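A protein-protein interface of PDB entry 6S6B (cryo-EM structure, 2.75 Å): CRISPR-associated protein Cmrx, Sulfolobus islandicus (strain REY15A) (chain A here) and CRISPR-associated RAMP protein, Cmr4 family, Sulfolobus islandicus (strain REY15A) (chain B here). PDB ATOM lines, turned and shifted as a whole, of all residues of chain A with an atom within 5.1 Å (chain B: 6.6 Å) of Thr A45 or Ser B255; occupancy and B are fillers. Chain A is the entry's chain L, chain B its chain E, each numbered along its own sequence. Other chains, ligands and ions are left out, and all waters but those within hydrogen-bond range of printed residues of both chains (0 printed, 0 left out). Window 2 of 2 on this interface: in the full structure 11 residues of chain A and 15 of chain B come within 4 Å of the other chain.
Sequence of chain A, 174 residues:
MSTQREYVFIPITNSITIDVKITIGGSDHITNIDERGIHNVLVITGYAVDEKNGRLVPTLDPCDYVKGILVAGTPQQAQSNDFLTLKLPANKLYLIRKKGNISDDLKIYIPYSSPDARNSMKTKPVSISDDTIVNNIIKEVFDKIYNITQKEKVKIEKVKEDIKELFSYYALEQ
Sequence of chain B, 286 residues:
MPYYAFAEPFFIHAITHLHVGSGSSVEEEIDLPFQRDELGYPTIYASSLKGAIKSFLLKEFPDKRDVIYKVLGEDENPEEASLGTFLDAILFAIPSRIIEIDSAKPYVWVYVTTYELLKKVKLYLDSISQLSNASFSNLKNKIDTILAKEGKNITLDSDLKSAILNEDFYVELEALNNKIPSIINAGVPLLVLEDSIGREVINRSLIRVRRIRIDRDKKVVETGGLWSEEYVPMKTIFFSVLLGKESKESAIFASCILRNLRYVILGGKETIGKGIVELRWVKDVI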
ATOM      1  N   VAL A  43      29.804  23.436 -31.158  1.00  0.00           N
ATOM      2  CA  VAL A  43      29.333  23.869 -29.848  1.00  0.00           C
ATOM      3  C   VAL A  43      29.187  22.631 -28.981  1.00  0.00           C
ATOM      4  O   VAL A  43      28.550  21.656 -29.391  1.00  0.00           O
ATOM      5  CB  VAL A  43      27.995  24.621 -29.915  1.00  0.00           C
ATOM      6  CG1 VAL A  43      27.550  25.034 -28.525  1.00  0.00           C
ATOM      7  CG2 VAL A  43      28.079  25.808 -30.847  1.00  0.00           C
ATOM      8  N   ILE A  44      29.773  22.664 -27.792  1.00  0.00           N
ATOM      9  CA  ILE A  44      29.685  21.564 -26.844  1.00  0.00           C
ATOM     10  C   ILE A  44      28.786  22.001 -25.701  1.00  0.00           C
ATOM     11  O   ILE A  44      29.081  22.984 -25.010  1.00  0.00           O
ATOM     12  CB  ILE A  44      31.073  21.150 -26.336  1.00  0.00           C
ATOM     13  CG1 ILE A  44      31.989  20.851 -27.520  1.00  0.00           C
ATOM     14  CG2 ILE A  44      30.964  19.949 -25.432  1.00  0.00           C
ATOM     15  CD1 ILE A  44      33.380  20.493 -27.122  1.00  0.00           C
ATOM     16  N   THR A  45      27.695  21.279 -25.499  1.00  0.00           N
ATOM     17  CA  THR A  45      26.680  21.652 -24.527  1.00  0.00           C
ATOM     18  C   THR A  45      26.917  20.920 -23.215  1.00  0.00           C
ATOM     19  O   THR A  45      27.208  19.722 -23.204  1.00  0.00           O
ATOM     20  CB  THR A  45      25.286  21.338 -25.068  1.00  0.00           C
ATOM     21  OG1 THR A  45      25.023  22.172 -26.203  1.00  0.00           O
ATOM     22  CG2 THR A  45      24.232  21.582 -24.020  1.00  0.00           C
ATOM     23  N   GLY A  46      26.790  21.648 -22.112  1.00  0.00           N
ATOM     24  CA  GLY A  46      27.051  21.108 -20.798  1.00  0.00           C
ATOM     25  C   GLY A  46      28.441  21.362 -20.266  1.00  0.00           C
ATOM     26  O   GLY A  46      28.811  20.771 -19.247  1.00  0.00           O
ATOM     27  N   TYR A  47      29.219  22.219 -20.919  1.00  0.00           N
ATOM     28  CA  TYR A  47      30.602  22.474 -20.552  1.00  0.00           C
ATOM     29  C   TYR A  47      30.831  23.973 -20.462  1.00  0.00           C
ATOM     30  O   TYR A  47      30.335  24.741 -21.286  1.00  0.00           O
ATOM     31  CB  TYR A  47      31.572  21.861 -21.572  1.00  0.00           C
ATOM     32  CG  TYR A  47      31.636  20.355 -21.526  1.00  0.00           C
ATOM     33  CD1 TYR A  47      30.569  19.583 -21.953  1.00  0.00           C
ATOM     34  CD2 TYR A  47      32.762  19.707 -21.054  1.00  0.00           C
ATOM     35  CE1 TYR A  47      30.620  18.213 -21.908  1.00  0.00           C
ATOM     36  CE2 TYR A  47      32.825  18.337 -21.007  1.00  0.00           C
ATOM     37  CZ  TYR A  47      31.751  17.593 -21.435  1.00  0.00           C
ATOM     38  OH  TYR A  47      31.812  16.220 -21.390  1.00  0.00           O
ATOM     39  N   ASP A  61      24.448  21.281 -16.537  1.00  0.00           N
ATOM     40  CA  ASP A  61      23.456  22.228 -17.020  1.00  0.00           C
ATOM     41  C   ASP A  61      23.399  22.174 -18.539  1.00  0.00           C
ATOM     42  O   ASP A  61      24.414  22.438 -19.195  1.00  0.00           O
ATOM     43  CB  ASP A  61      23.814  23.631 -16.542  1.00  0.00           C
ATOM     44  CG  ASP A  61      22.695  24.637 -16.751  1.00  0.00           C
ATOM     45  OD1 ASP A  61      21.806  24.385 -17.589  1.00  0.00           O
ATOM     46  OD2 ASP A  61      22.707  25.689 -16.080  1.00  0.00           O
ATOM     47  N   PRO A  62      22.255  21.841 -19.137  1.00  0.00           N
ATOM     48  CA  PRO A  62      22.164  21.879 -20.602  1.00  0.00           C
ATOM     49  C   PRO A  62      22.205  23.280 -21.173  1.00  0.00           C
ATOM     50  O   PRO A  62      22.242  23.426 -22.399  1.00  0.00           O
ATOM     51  CB  PRO A  62      20.821  21.199 -20.891  1.00  0.00           C
ATOM     52  CG  PRO A  62      20.054  21.317 -19.636  1.00  0.00           C
ATOM     53  CD  PRO A  62      21.035  21.306 -18.517  1.00  0.00           C
ATOM     54  N   CYS A  63      22.199  24.315 -20.332  1.00  0.00           N
ATOM     55  CA  CYS A  63      22.292  25.677 -20.839  1.00  0.00           C
ATOM     56  C   CYS A  63      23.730  26.117 -21.050  1.00  0.00           C
ATOM     57  O   CYS A  63      23.989  26.919 -21.950  1.00  0.00           O
ATOM     58  CB  CYS A  63      21.587  26.647 -19.893  1.00  0.00           C
ATOM     59  SG  CYS A  63      19.919  26.148 -19.412  1.00  0.00           S
ATOM     60  N   ASP A  64      24.664  25.616 -20.250  1.00  0.00           N
ATOM     61  CA  ASP A  64      26.062  25.994 -20.390  1.00  0.00           C
ATOM     62  C   ASP A  64      26.645  25.359 -21.641  1.00  0.00           C
ATOM     63  O   ASP A  64      26.503  24.153 -21.856  1.00  0.00           O
ATOM     64  CB  ASP A  64      26.856  25.564 -19.161  1.00  0.00           C
ATOM     65  CG  ASP A  64      26.362  26.220 -17.895  1.00  0.00           C
ATOM     66  OD1 ASP A  64      26.085  27.433 -17.923  1.00  0.00           O
ATOM     67  OD2 ASP A  64      26.260  25.527 -16.866  1.00  0.00           O
ATOM     68  N   TYR A  65      27.307  26.167 -22.461  1.00  0.00           N
ATOM     69  CA  TYR A  65      27.864  25.664 -23.706  1.00  0.00           C
ATOM     70  C   TYR A  65      29.102  26.470 -24.065  1.00  0.00           C
ATOM     71  O   TYR A  65      29.310  27.582 -23.574  1.00  0.00           O
ATOM     72  CB  TYR A  65      26.834  25.721 -24.837  1.00  0.00           C
ATOM     73  CG  TYR A  65      26.507  27.125 -25.261  1.00  0.00           C
ATOM     74  CD1 TYR A  65      25.462  27.818 -24.680  1.00  0.00           C
ATOM     75  CD2 TYR A  65      27.249  27.762 -26.238  1.00  0.00           C
ATOM     76  CE1 TYR A  65      25.167  29.104 -25.059  1.00  0.00           C
ATOM     77  CE2 TYR A  65      26.962  29.037 -26.620  1.00  0.00           C
ATOM     78  CZ  TYR A  65      25.922  29.708 -26.031  1.00  0.00           C
ATOM     79  OH  TYR A  65      25.639  30.994 -26.422  1.00  0.00           O
ATOM     80  N   TYR A  94      27.148  18.857 -33.027  1.00  0.00           N
ATOM     81  CA  TYR A  94      26.277  20.023 -33.030  1.00  0.00           C
ATOM     82  C   TYR A  94      27.069  21.146 -33.693  1.00  0.00           C
ATOM     83  O   TYR A  94      27.755  21.920 -33.027  1.00  0.00           O
ATOM     84  CB  TYR A  94      25.847  20.380 -31.616  1.00  0.00           C
ATOM     85  CG  TYR A  94      25.007  21.631 -31.515  1.00  0.00           C
ATOM     86  CD1 TYR A  94      23.657  21.621 -31.800  1.00  0.00           C
ATOM     87  CD2 TYR A  94      25.575  22.826 -31.141  1.00  0.00           C
ATOM     88  CE1 TYR A  94      22.906  22.778 -31.700  1.00  0.00           C
ATOM     89  CE2 TYR A  94      24.836  23.979 -31.044  1.00  0.00           C
ATOM     90  CZ  TYR A  94      23.505  23.954 -31.324  1.00  0.00           C
ATOM     91  OH  TYR A  94      22.773  25.114 -31.223  1.00  0.00           O
ATOM     92  N   SER B 250      14.326  24.765 -22.884  1.00  0.00           N
ATOM     93  CA  SER B 250      14.607  25.631 -24.017  1.00  0.00           C
ATOM     94  C   SER B 250      16.013  25.397 -24.541  1.00  0.00           C
ATOM     95  O   SER B 250      16.266  25.524 -25.743  1.00  0.00           O
ATOM     96  CB  SER B 250      14.427  27.088 -23.611  1.00  0.00           C
ATOM     97  OG  SER B 250      13.251  27.252 -22.844  1.00  0.00           O
ATOM     98  N   ALA B 251      16.944  25.065 -23.649  1.00  0.00           N
ATOM     99  CA  ALA B 251      18.301  24.759 -24.077  1.00  0.00           C
ATOM    100  C   ALA B 251      18.330  23.509 -24.942  1.00  0.00           C
ATOM    101  O   ALA B 251      18.963  23.487 -26.001  1.00  0.00           O
ATOM    102  CB  ALA B 251      19.203  24.596 -22.857  1.00  0.00           C
ATOM    103  N   ILE B 252      17.646  22.453 -24.504  1.00  0.00           N
ATOM    104  CA  ILE B 252      17.594  21.224 -25.287  1.00  0.00           C
ATOM    105  C   ILE B 252      16.859  21.462 -26.595  1.00  0.00           C
ATOM    106  O   ILE B 252      17.304  21.037 -27.667  1.00  0.00           O
ATOM    107  CB  ILE B 252      16.927  20.102 -24.478  1.00  0.00           C
ATOM    108  CG1 ILE B 252      17.842  19.648 -23.352  1.00  0.00           C
ATOM    109  CG2 ILE B 252      16.580  18.936 -25.375  1.00  0.00           C
ATOM    110  CD1 ILE B 252      17.260  18.530 -22.570  1.00  0.00           C
ATOM    111  N   PHE B 253      15.706  22.127 -26.518  1.00  0.00           N
ATOM    112  CA  PHE B 253      14.940  22.457 -27.710  1.00  0.00           C
ATOM    113  C   PHE B 253      15.811  23.147 -28.749  1.00  0.00           C
ATOM    114  O   PHE B 253      15.838  22.752 -29.918  1.00  0.00           O
ATOM    115  CB  PHE B 253      13.759  23.341 -27.325  1.00  0.00           C
ATOM    116  CG  PHE B 253      12.660  23.359 -28.336  1.00  0.00           C
ATOM    117  CD1 PHE B 253      11.681  22.389 -28.324  1.00  0.00           C
ATOM    118  CD2 PHE B 253      12.598  24.353 -29.288  1.00  0.00           C
ATOM    119  CE1 PHE B 253      10.670  22.407 -29.247  1.00  0.00           C
ATOM    120  CE2 PHE B 253      11.587  24.373 -30.207  1.00  0.00           C
ATOM    121  CZ  PHE B 253      10.624  23.398 -30.189  1.00  0.00           C
ATOM    122  N   ALA B 254      16.543  24.177 -28.335  1.00  0.00           N
ATOM    123  CA  ALA B 254      17.376  24.905 -29.284  1.00  0.00           C
ATOM    124  C   ALA B 254      18.542  24.064 -29.774  1.00  0.00           C
ATOM    125  O   ALA B 254      18.992  24.238 -30.909  1.00  0.00           O
ATOM    126  CB  ALA B 254      17.889  26.195 -28.651  1.00  0.00           C
ATOM    127  N   SER B 255      19.041  23.150 -28.947  1.00  0.00           N
ATOM    128  CA  SER B 255      20.271  22.441 -29.270  1.00  0.00           C
ATOM    129  C   SER B 255      20.037  21.070 -29.879  1.00  0.00           C
ATOM    130  O   SER B 255      20.907  20.565 -30.594  1.00  0.00           O
ATOM    131  CB  SER B 255      21.134  22.293 -28.019  1.00  0.00           C
ATOM    132  OG  SER B 255      21.844  23.488 -27.760  1.00  0.00           O
ATOM    133  N   CYS B 256      18.891  20.452 -29.620  1.00  0.00           N
ATOM    134  CA  CYS B 256      18.606  19.138 -30.164  1.00  0.00           C
ATOM    135  C   CYS B 256      17.493  19.126 -31.195  1.00  0.00           C
ATOM    136  O   CYS B 256      17.626  18.435 -32.208  1.00  0.00           O
ATOM    137  CB  CYS B 256      18.242  18.158 -29.040  1.00  0.00           C
ATOM    138  SG  CYS B 256      17.762  16.521 -29.613  1.00  0.00           S
ATOM    139  N   ILE B 257      16.414  19.871 -30.981  1.00  0.00           N
ATOM    140  CA  ILE B 257      15.264  19.773 -31.867  1.00  0.00           C
ATOM    141  C   ILE B 257      15.410  20.707 -33.056  1.00  0.00           C
ATOM    142  O   ILE B 257      15.121  20.330 -34.195  1.00  0.00           O
ATOM    143  CB  ILE B 257      13.973  20.054 -31.087  1.00  0.00           C
ATOM    144  CG1 ILE B 257      13.962  19.261 -29.785  1.00  0.00           C
ATOM    145  CG2 ILE B 257      12.775  19.693 -31.921  1.00  0.00           C
ATOM    146  CD1 ILE B 257      13.889  17.784 -29.990  1.00  0.00           C
ATOM    147  N   LEU B 258      15.856  21.935 -32.819  1.00  0.00           N
ATOM    148  CA  LEU B 258      15.895  22.923 -33.889  1.00  0.00           C
ATOM    149  C   LEU B 258      17.020  22.697 -34.877  1.00  0.00           C
ATOM    150  O   LEU B 258      17.120  23.453 -35.847  1.00  0.00           O
ATOM    151  CB  LEU B 258      16.008  24.328 -33.307  1.00  0.00           C
ATOM    152  CG  LEU B 258      14.796  24.790 -32.512  1.00  0.00           C
ATOM    153  CD1 LEU B 258      14.737  26.297 -32.492  1.00  0.00           C
ATOM    154  CD2 LEU B 258      13.528  24.219 -33.108  1.00  0.00           C
ATOM    155  N   ARG B 259      17.871  21.702 -34.663  1.00  0.00           N
ATOM    156  CA  ARG B 259      18.889  21.353 -35.638  1.00  0.00           C
ATOM    157  C   ARG B 259      18.523  20.116 -36.437  1.00  0.00           C
ATOM    158  O   ARG B 259      19.194  19.814 -37.427  1.00  0.00           O
ATOM    159  CB  ARG B 259      20.232  21.140 -34.943  1.00  0.00           C
ATOM    160  CG  ARG B 259      20.477  22.122 -33.827  1.00  0.00           C
ATOM    161  CD  ARG B 259      20.540  23.548 -34.335  1.00  0.00           C
ATOM    162  NE  ARG B 259      21.767  23.810 -35.077  1.00  0.00           N
ATOM    163  CZ  ARG B 259      21.846  24.636 -36.113  1.00  0.00           C
ATOM    164  NH1 ARG B 259      20.766  25.276 -36.531  1.00  0.00           N
ATOM    165  NH2 ARG B 259      23.001  24.820 -36.734  1.00  0.00           N
ATOM    166  N   ASN B 260      17.473  19.410 -36.037  1.00  0.00           N
ATOM    167  CA  ASN B 260      16.936  18.294 -36.797  1.00  0.00           C
ATOM    168  C   ASN B 260      15.608  18.643 -37.445  1.00  0.00           C
ATOM    169  O   ASN B 260      14.915  17.753 -37.944  1.00  0.00           O
ATOM    170  CB  ASN B 260      16.787  17.073 -35.893  1.00  0.00           C
ATOM    171  CG  ASN B 260      17.984  16.879 -34.996  1.00  0.00           C
ATOM    172  OD1 ASN B 260      19.119  17.101 -35.407  1.00  0.00           O
ATOM    173  ND2 ASN B 260      17.736  16.465 -33.763  1.00  0.00           N
ATOM    174  N   LYS B 283      20.743  31.237 -38.369  1.00  0.00           N
ATOM    175  CA  LYS B 283      22.019  31.055 -37.690  1.00  0.00           C
ATOM    176  C   LYS B 283      23.014  30.290 -38.547  1.00  0.00           C
ATOM    177  O   LYS B 283      24.227  30.452 -38.377  1.00  0.00           O
ATOM    178  CB  LYS B 283      21.809  30.338 -36.359  1.00  0.00           C
ATOM    179  CG  LYS B 283      21.740  28.835 -36.472  1.00  0.00           C
ATOM    180  CD  LYS B 283      21.210  28.217 -35.200  1.00  0.00           C
ATOM    181  CE  LYS B 283      22.095  28.549 -34.014  1.00  0.00           C
ATOM    182  NZ  LYS B 283      21.714  27.750 -32.822  1.00  0.00           N
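Hydrophobic or aromatic side chains of chain B that line the printed part of chain A: Ala B251. Of the 11 printed residues of chain A, 4 touch a printed residue of chain B. Hydrophobic or aromatic side chains of chain A that line the printed part of chain B: Tyr A94. Among the printed residues, 7 pairs touch across the chains. Among the printed residues, no Asp or Glu carboxylate lies within 4 Å of a Lys or Arg side-chain nitrogen of the other chain.
Of chain B, only Ser B255 comes within 4 Å of Thr A45. Of chain A, only Thr A45 (3.8 Å) and Tyr A94 (3.2 Å) come within 4 Å of Ser B255. Of the printed residues of chain A, Ala B254 touches Tyr A94. Of the printed residues of chain A, Ala B251 touches Pro A62 and Cys A63. The nearest printed residue of chain A that does not touch Ser B255 is Pro A62 (5.4 Å). The nearest printed residue of chain B that does not touch Pro A62 is Ile B252 (4.2 Å).
Among the printed residues, merely in contact across the chains: Thr A45 with Ser B255 (3.8 Å), Pro A62 with Ala B251 (3.3 Å), Cys A63 with Ala B251 (3.8 Å), Tyr A94 with Ala B254 (3.9 Å), Tyr A94 with Ser B255 (3.2 Å) and Tyr A94 with Arg B259 (3.3 Å).
The side-chain carboxylate (OD1) of Asp A61 is in hydrogen-bond range of the backbone NH (N) of Cys A63, 2.8 Å away. The backbone carbonyl oxygen of Tyr A94 is in hydrogen-bond range of the backbone NH of Val A43, 3.2 Å away. The backbone carbonyl oxygen of Ala B251 lies close to the side-chain hydroxyl of Ser B255, at 3.4 Å.
NZ of Lys B283 is in hydrogen-bond range of OH of Tyr A94, 3.3 Å away.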
